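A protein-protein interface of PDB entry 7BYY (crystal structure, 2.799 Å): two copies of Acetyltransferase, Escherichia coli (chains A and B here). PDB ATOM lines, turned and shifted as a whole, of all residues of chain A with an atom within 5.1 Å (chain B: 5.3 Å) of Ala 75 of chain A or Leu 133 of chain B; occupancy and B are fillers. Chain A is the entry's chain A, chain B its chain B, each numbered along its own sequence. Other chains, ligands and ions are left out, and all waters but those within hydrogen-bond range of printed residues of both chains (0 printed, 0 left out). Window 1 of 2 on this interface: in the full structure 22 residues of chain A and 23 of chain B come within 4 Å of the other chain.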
ATOM      1  N   PHE A  73      -8.842 -16.027 -16.484  1.00  0.00           N
ATOM      2  CA  PHE A  73      -9.895 -16.835 -17.081  1.00  0.00           C
ATOM      3  C   PHE A  73      -9.330 -17.587 -18.278  1.00  0.00           C
ATOM      4  O   PHE A  73      -8.377 -17.134 -18.918  1.00  0.00           O
ATOM      5  CB  PHE A  73     -11.082 -15.964 -17.501  1.00  0.00           C
ATOM      6  CG  PHE A  73     -10.689 -14.751 -18.294  1.00  0.00           C
ATOM      7  CD1 PHE A  73     -10.283 -13.589 -17.656  1.00  0.00           C
ATOM      8  CD2 PHE A  73     -10.724 -14.773 -19.679  1.00  0.00           C
ATOM      9  CE1 PHE A  73      -9.919 -12.472 -18.385  1.00  0.00           C
ATOM     10  CE2 PHE A  73     -10.365 -13.658 -20.412  1.00  0.00           C
ATOM     11  CZ  PHE A  73      -9.962 -12.505 -19.763  1.00  0.00           C
ATOM     12  N   THR A  74      -9.922 -18.748 -18.560  1.00  0.00           N
ATOM     13  CA  THR A  74      -9.506 -19.620 -19.653  1.00  0.00           C
ATOM     14  C   THR A  74     -10.732 -20.056 -20.445  1.00  0.00           C
ATOM     15  O   THR A  74     -11.866 -19.676 -20.142  1.00  0.00           O
ATOM     16  CB  THR A  74      -8.758 -20.860 -19.140  1.00  0.00           C
ATOM     17  OG1 THR A  74      -9.699 -21.792 -18.590  1.00  0.00           O
ATOM     18  CG2 THR A  74      -7.748 -20.491 -18.069  1.00  0.00           C
ATOM     19  N   ALA A  75     -10.498 -20.868 -21.470  1.00  0.00           N
ATOM     20  CA  ALA A  75     -11.578 -21.535 -22.182  1.00  0.00           C
ATOM     21  C   ALA A  75     -11.840 -22.897 -21.551  1.00  0.00           C
ATOM     22  O   ALA A  75     -10.926 -23.553 -21.044  1.00  0.00           O
ATOM     23  CB  ALA A  75     -11.243 -21.694 -23.666  1.00  0.00           C
ATOM     24  N   TYR A  76     -13.101 -23.318 -21.584  1.00  0.00           N
ATOM     25  CA  TYR A  76     -13.508 -24.505 -20.850  1.00  0.00           C
ATOM     26  C   TYR A  76     -14.773 -25.067 -21.481  1.00  0.00           C
ATOM     27  O   TYR A  76     -15.533 -24.351 -22.136  1.00  0.00           O
ATOM     28  CB  TYR A  76     -13.734 -24.181 -19.369  1.00  0.00           C
ATOM     29  CG  TYR A  76     -13.750 -25.381 -18.451  1.00  0.00           C
ATOM     30  CD1 TYR A  76     -12.810 -26.394 -18.582  1.00  0.00           C
ATOM     31  CD2 TYR A  76     -14.698 -25.493 -17.443  1.00  0.00           C
ATOM     32  CE1 TYR A  76     -12.822 -27.490 -17.738  1.00  0.00           C
ATOM     33  CE2 TYR A  76     -14.716 -26.581 -16.594  1.00  0.00           C
ATOM     34  CZ  TYR A  76     -13.777 -27.578 -16.747  1.00  0.00           C
ATOM     35  OH  TYR A  76     -13.794 -28.666 -15.904  1.00  0.00           O
ATOM     36  N   SER A  77     -14.986 -26.365 -21.277  1.00  0.00           N
ATOM     37  CA  SER A  77     -16.164 -27.043 -21.797  1.00  0.00           C
ATOM     38  C   SER A  77     -16.718 -27.975 -20.731  1.00  0.00           C
ATOM     39  O   SER A  77     -15.959 -28.600 -19.986  1.00  0.00           O
ATOM     40  CB  SER A  77     -15.845 -27.830 -23.078  1.00  0.00           C
ATOM     41  OG  SER A  77     -14.983 -28.924 -22.814  1.00  0.00           O
ATOM     42  N   VAL A  97     -17.982 -22.839 -22.554  1.00  0.00           N
ATOM     43  CA  VAL A  97     -18.135 -21.684 -21.676  1.00  0.00           C
ATOM     44  C   VAL A  97     -16.769 -21.053 -21.442  1.00  0.00           C
ATOM     45  O   VAL A  97     -15.728 -21.617 -21.781  1.00  0.00           O
ATOM     46  CB  VAL A  97     -18.775 -22.045 -20.315  1.00  0.00           C
ATOM     47  CG1 VAL A  97     -20.174 -22.628 -20.495  1.00  0.00           C
ATOM     48  CG2 VAL A  97     -17.870 -22.993 -19.537  1.00  0.00           C
ATOM     49  N   VAL A  98     -16.786 -19.870 -20.839  1.00  0.00           N
ATOM     50  CA  VAL A  98     -15.578 -19.227 -20.340  1.00  0.00           C
ATOM     51  C   VAL A  98     -15.515 -19.470 -18.840  1.00  0.00           C
ATOM     52  O   VAL A  98     -16.456 -19.135 -18.111  1.00  0.00           O
ATOM     53  CB  VAL A  98     -15.561 -17.726 -20.662  1.00  0.00           C
ATOM     54  CG1 VAL A  98     -14.463 -17.031 -19.868  1.00  0.00           C
ATOM     55  CG2 VAL A  98     -15.369 -17.508 -22.157  1.00  0.00           C
ATOM     56  N   ARG A  99     -14.420 -20.060 -18.370  1.00  0.00           N
ATOM     57  CA  ARG A  99     -14.269 -20.341 -16.950  1.00  0.00           C
ATOM     58  C   ARG A  99     -13.545 -19.193 -16.260  1.00  0.00           C
ATOM     59  O   ARG A  99     -12.480 -18.760 -16.711  1.00  0.00           O
ATOM     60  CB  ARG A  99     -13.510 -21.646 -16.712  1.00  0.00           C
ATOM     61  CG  ARG A  99     -13.259 -21.910 -15.235  1.00  0.00           C
ATOM     62  CD  ARG A  99     -12.554 -23.225 -14.994  1.00  0.00           C
ATOM     63  NE  ARG A  99     -11.436 -23.412 -15.907  1.00  0.00           N
ATOM     64  CZ  ARG A  99     -10.396 -24.201 -15.661  1.00  0.00           C
ATOM     65  NH1 ARG A  99     -10.332 -24.873 -14.517  1.00  0.00           N
ATOM     66  NH2 ARG A  99      -9.421 -24.313 -16.559  1.00  0.00           N
ATOM     67  N   HIS A 125     -15.528  -8.137 -21.293  1.00  0.00           N
ATOM     68  CA  HIS A 125     -14.595  -8.929 -22.082  1.00  0.00           C
ATOM     69  C   HIS A 125     -15.227 -10.234 -22.548  1.00  0.00           C
ATOM     70  O   HIS A 125     -14.926 -10.708 -23.652  1.00  0.00           O
ATOM     71  CB  HIS A 125     -13.329  -9.208 -21.278  1.00  0.00           C
ATOM     72  CG  HIS A 125     -12.172  -9.650 -22.115  1.00  0.00           C
ATOM     73  ND1 HIS A 125     -11.484  -8.790 -22.944  1.00  0.00           N
ATOM     74  CD2 HIS A 125     -11.590 -10.862 -22.263  1.00  0.00           C
ATOM     75  CE1 HIS A 125     -10.521  -9.453 -23.559  1.00  0.00           C
ATOM     76  NE2 HIS A 125     -10.564 -10.713 -23.164  1.00  0.00           N
ATOM     77  N   ILE A 129     -15.550 -11.918 -26.282  1.00  0.00           N
ATOM     78  CA  ILE A 129     -15.264 -13.315 -26.590  1.00  0.00           C
ATOM     79  C   ILE A 129     -16.461 -13.965 -27.271  1.00  0.00           C
ATOM     80  O   ILE A 129     -16.308 -14.748 -28.218  1.00  0.00           O
ATOM     81  CB  ILE A 129     -14.860 -14.064 -25.308  1.00  0.00           C
ATOM     82  CG1 ILE A 129     -13.542 -13.496 -24.772  1.00  0.00           C
ATOM     83  CG2 ILE A 129     -14.771 -15.559 -25.566  1.00  0.00           C
ATOM     84  CD1 ILE A 129     -13.151 -14.017 -23.410  1.00  0.00           C
ATOM     85  N   TYR B  76     -14.157 -25.452 -26.861  1.00  0.00           N
ATOM     86  CA  TYR B  76     -13.983 -26.826 -26.421  1.00  0.00           C
ATOM     87  C   TYR B  76     -12.834 -26.890 -25.426  1.00  0.00           C
ATOM     88  O   TYR B  76     -12.127 -25.906 -25.191  1.00  0.00           O
ATOM     89  CB  TYR B  76     -13.728 -27.758 -27.614  1.00  0.00           C
ATOM     90  CG  TYR B  76     -14.022 -29.216 -27.349  1.00  0.00           C
ATOM     91  CD1 TYR B  76     -15.323 -29.659 -27.162  1.00  0.00           C
ATOM     92  CD2 TYR B  76     -12.998 -30.152 -27.294  1.00  0.00           C
ATOM     93  CE1 TYR B  76     -15.596 -30.993 -26.922  1.00  0.00           C
ATOM     94  CE2 TYR B  76     -13.259 -31.488 -27.054  1.00  0.00           C
ATOM     95  CZ  TYR B  76     -14.560 -31.904 -26.867  1.00  0.00           C
ATOM     96  OH  TYR B  76     -14.827 -33.235 -26.627  1.00  0.00           O
ATOM     97  N   SER B  77     -12.654 -28.066 -24.833  1.00  0.00           N
ATOM     98  CA  SER B  77     -11.564 -28.287 -23.896  1.00  0.00           C
ATOM     99  C   SER B  77     -11.207 -29.763 -23.893  1.00  0.00           C
ATOM    100  O   SER B  77     -12.087 -30.623 -23.989  1.00  0.00           O
ATOM    101  CB  SER B  77     -11.931 -27.834 -22.479  1.00  0.00           C
ATOM    102  OG  SER B  77     -12.557 -28.883 -21.760  1.00  0.00           O
ATOM    103  N   ILE B  95      -6.997 -28.538 -21.001  1.00  0.00           N
ATOM    104  CA  ILE B  95      -6.464 -27.683 -22.053  1.00  0.00           C
ATOM    105  C   ILE B  95      -7.620 -26.997 -22.772  1.00  0.00           C
ATOM    106  O   ILE B  95      -8.703 -27.565 -22.934  1.00  0.00           O
ATOM    107  CB  ILE B  95      -5.576 -28.505 -23.015  1.00  0.00           C
ATOM    108  CG1 ILE B  95      -4.398 -27.666 -23.503  1.00  0.00           C
ATOM    109  CG2 ILE B  95      -6.373 -29.060 -24.187  1.00  0.00           C
ATOM    110  CD1 ILE B  95      -3.532 -27.142 -22.381  1.00  0.00           C
ATOM    111  N   GLY B  96      -7.405 -25.749 -23.181  1.00  0.00           N
ATOM    112  CA  GLY B  96      -8.433 -24.994 -23.875  1.00  0.00           C
ATOM    113  C   GLY B  96      -8.145 -24.844 -25.356  1.00  0.00           C
ATOM    114  O   GLY B  96      -7.085 -24.335 -25.736  1.00  0.00           O
ATOM    115  N   VAL B  97      -9.073 -25.286 -26.205  1.00  0.00           N
ATOM    116  CA  VAL B  97      -8.865 -25.320 -27.648  1.00  0.00           C
ATOM    117  C   VAL B  97     -10.098 -24.764 -28.353  1.00  0.00           C
ATOM    118  O   VAL B  97     -11.125 -24.484 -27.737  1.00  0.00           O
ATOM    119  CB  VAL B  97      -8.560 -26.744 -28.160  1.00  0.00           C
ATOM    120  CG1 VAL B  97      -7.297 -27.292 -27.515  1.00  0.00           C
ATOM    121  CG2 VAL B  97      -9.748 -27.663 -27.906  1.00  0.00           C
ATOM    122  N   ILE B 129      -9.778 -14.886 -32.159  1.00  0.00           N
ATOM    123  CA  ILE B 129     -10.232 -15.482 -30.907  1.00  0.00           C
ATOM    124  C   ILE B 129      -9.088 -15.549 -29.905  1.00  0.00           C
ATOM    125  O   ILE B 129      -9.262 -15.250 -28.716  1.00  0.00           O
ATOM    126  CB  ILE B 129     -10.831 -16.877 -31.166  1.00  0.00           C
ATOM    127  CG1 ILE B 129     -12.056 -16.780 -32.076  1.00  0.00           C
ATOM    128  CG2 ILE B 129     -11.188 -17.557 -29.852  1.00  0.00           C
ATOM    129  CD1 ILE B 129     -12.636 -18.127 -32.455  1.00  0.00           C
ATOM    130  N   HIS B 130      -7.896 -15.929 -30.373  1.00  0.00           N
ATOM    131  CA  HIS B 130      -6.755 -16.098 -29.477  1.00  0.00           C
ATOM    132  C   HIS B 130      -6.364 -14.787 -28.808  1.00  0.00           C
ATOM    133  O   HIS B 130      -5.863 -14.796 -27.677  1.00  0.00           O
ATOM    134  CB  HIS B 130      -5.572 -16.681 -30.253  1.00  0.00           C
ATOM    135  CG  HIS B 130      -4.365 -16.949 -29.410  1.00  0.00           C
ATOM    136  ND1 HIS B 130      -4.306 -17.980 -28.497  1.00  0.00           N
ATOM    137  CD2 HIS B 130      -3.165 -16.322 -29.347  1.00  0.00           C
ATOM    138  CE1 HIS B 130      -3.125 -17.975 -27.906  1.00  0.00           C
ATOM    139  NE2 HIS B 130      -2.414 -16.979 -28.404  1.00  0.00           N
ATOM    140  N   GLN B 131      -6.592 -13.657 -29.478  1.00  0.00           N
ATOM    141  CA  GLN B 131      -6.259 -12.355 -28.913  1.00  0.00           C
ATOM    142  C   GLN B 131      -7.269 -11.882 -27.873  1.00  0.00           C
ATOM    143  O   GLN B 131      -7.004 -10.891 -27.184  1.00  0.00           O
ATOM    144  CB  GLN B 131      -6.129 -11.320 -30.032  1.00  0.00           C
ATOM    145  CG  GLN B 131      -5.062 -11.692 -31.055  1.00  0.00           C
ATOM    146  CD  GLN B 131      -4.856 -10.638 -32.128  1.00  0.00           C
ATOM    147  OE1 GLN B 131      -5.624  -9.681 -32.239  1.00  0.00           O
ATOM    148  NE2 GLN B 131      -3.811 -10.814 -32.927  1.00  0.00           N
ATOM    149  N   ALA B 132      -8.406 -12.563 -27.739  1.00  0.00           N
ATOM    150  CA  ALA B 132      -9.368 -12.271 -26.686  1.00  0.00           C
ATOM    151  C   ALA B 132      -9.472 -13.377 -25.653  1.00  0.00           C
ATOM    152  O   ALA B 132      -9.661 -13.087 -24.469  1.00  0.00           O
ATOM    153  CB  ALA B 132     -10.758 -12.018 -27.280  1.00  0.00           C
ATOM    154  N   LEU B 133      -9.347 -14.633 -26.080  1.00  0.00           N
ATOM    155  CA  LEU B 133      -9.402 -15.788 -25.186  1.00  0.00           C
ATOM    156  C   LEU B 133      -8.267 -16.723 -25.584  1.00  0.00           C
ATOM    157  O   LEU B 133      -8.371 -17.443 -26.589  1.00  0.00           O
ATOM    158  CB  LEU B 133     -10.755 -16.489 -25.269  1.00  0.00           C
ATOM    159  CG  LEU B 133     -10.990 -17.620 -24.273  1.00  0.00           C
ATOM    160  CD1 LEU B 133     -10.831 -17.105 -22.853  1.00  0.00           C
ATOM    161  CD2 LEU B 133     -12.365 -18.231 -24.476  1.00  0.00           C
ATOM    162  N   PRO B 134      -7.163 -16.719 -24.840  1.00  0.00           N
ATOM    163  CA  PRO B 134      -6.001 -17.537 -25.222  1.00  0.00           C
ATOM    164  C   PRO B 134      -6.340 -19.017 -25.304  1.00  0.00           C
ATOM    165  O   PRO B 134      -6.929 -19.594 -24.389  1.00  0.00           O
ATOM    166  CB  PRO B 134      -4.990 -17.252 -24.106  1.00  0.00           C
ATOM    167  CG  PRO B 134      -5.351 -15.882 -23.635  1.00  0.00           C
ATOM    168  CD  PRO B 134      -6.853 -15.804 -23.732  1.00  0.00           C
ATOM    169  N   ILE B 135      -5.952 -19.628 -26.421  1.00  0.00           N
ATOM    170  CA  ILE B 135      -6.171 -21.041 -26.677  1.00  0.00           C
ATOM    171  C   ILE B 135      -4.828 -21.683 -26.999  1.00  0.00           C
ATOM    172  O   ILE B 135      -3.848 -21.008 -27.324  1.00  0.00           O
ATOM    173  CB  ILE B 135      -7.169 -21.272 -27.826  1.00  0.00           C
ATOM    174  CG1 ILE B 135      -6.819 -20.361 -29.006  1.00  0.00           C
ATOM    175  CG2 ILE B 135      -8.594 -21.031 -27.350  1.00  0.00           C
ATOM    176  CD1 ILE B 135      -7.775 -20.463 -30.158  1.00  0.00           C
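Phe 73 of chain A touches Leu 133 of chain B. C of Thr 74 of chain A touches CD1 of Leu 133 of chain B, 3.8 Å away. Ala 75 of chain A touches Leu 133 of chain B (CB to CD2, 3.7 Å). Ser 77 of chain A touches Tyr 76 of chain B (CB to C, 3.9 Å). Leu 133 of chain B touches Val 98 of chain A. Ile 129 of chain A touches Ala 132 of chain B. Ile 129 of chain A touches Leu 133 of chain B.
Of chain B, only Leu 133 comes within 4 Å of Ala 75 of chain A. Of the printed residues of chain B, Thr 74 of chain A touches Leu 133. Of the printed residues of chain B, Ile 129 of chain A touches Ala 132 and Leu 133. Of the printed residues of chain B, His 125 of chain A touches Ala 132 (2.9 Å). Of the printed residues of chain A, Ala 132 of chain B touches His 125 and Ile 129.
Ser 77 of chain A touches Tyr 76 of chain B, but with the chains exchanged Tyr 76 of chain A does not touch Ser 77 of chain B (4.03 Å). Ser 77 of chain B touches its own counterpart, Ser 77 of chain A. Positions printed for both chains: 76, 77, 97 and 129. Of the 9 pairs that touch across the chains among the printed residues, 1 has its exchanged pair printed and touching as well.
The backbone carbonyl oxygen (O) of Ala 132 of chain B sits at hydrogen-bond distance from a ring nitrogen (NE2) of His 125 of chain A. The side-chain hydroxyl of Ser 77 of chain A is in hydrogen-bond range of the side-chain hydroxyl of Ser 77 of chain B (2.6 Å).
Hydrophobic or aromatic side chains of chain B that line the printed part of chain A: Leu 133. Of the 10 printed residues of chain A, 7 touch a printed residue of chain B. Among the printed residues, 9 pairs touch across the chains. Among the printed residues, no Asp or Glu carboxylate lies within 4 Å of a Lys or Arg side-chain nitrogen of the other chain.
The backbone NH (N) of Arg 99 of chain A is in hydrogen-bond range of the backbone carbonyl oxygen (O) of Thr 74 of chain A. N of Val 97 of chain B lies within hydrogen-bond range of O of Tyr 76 of chain B (3.3 Å).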
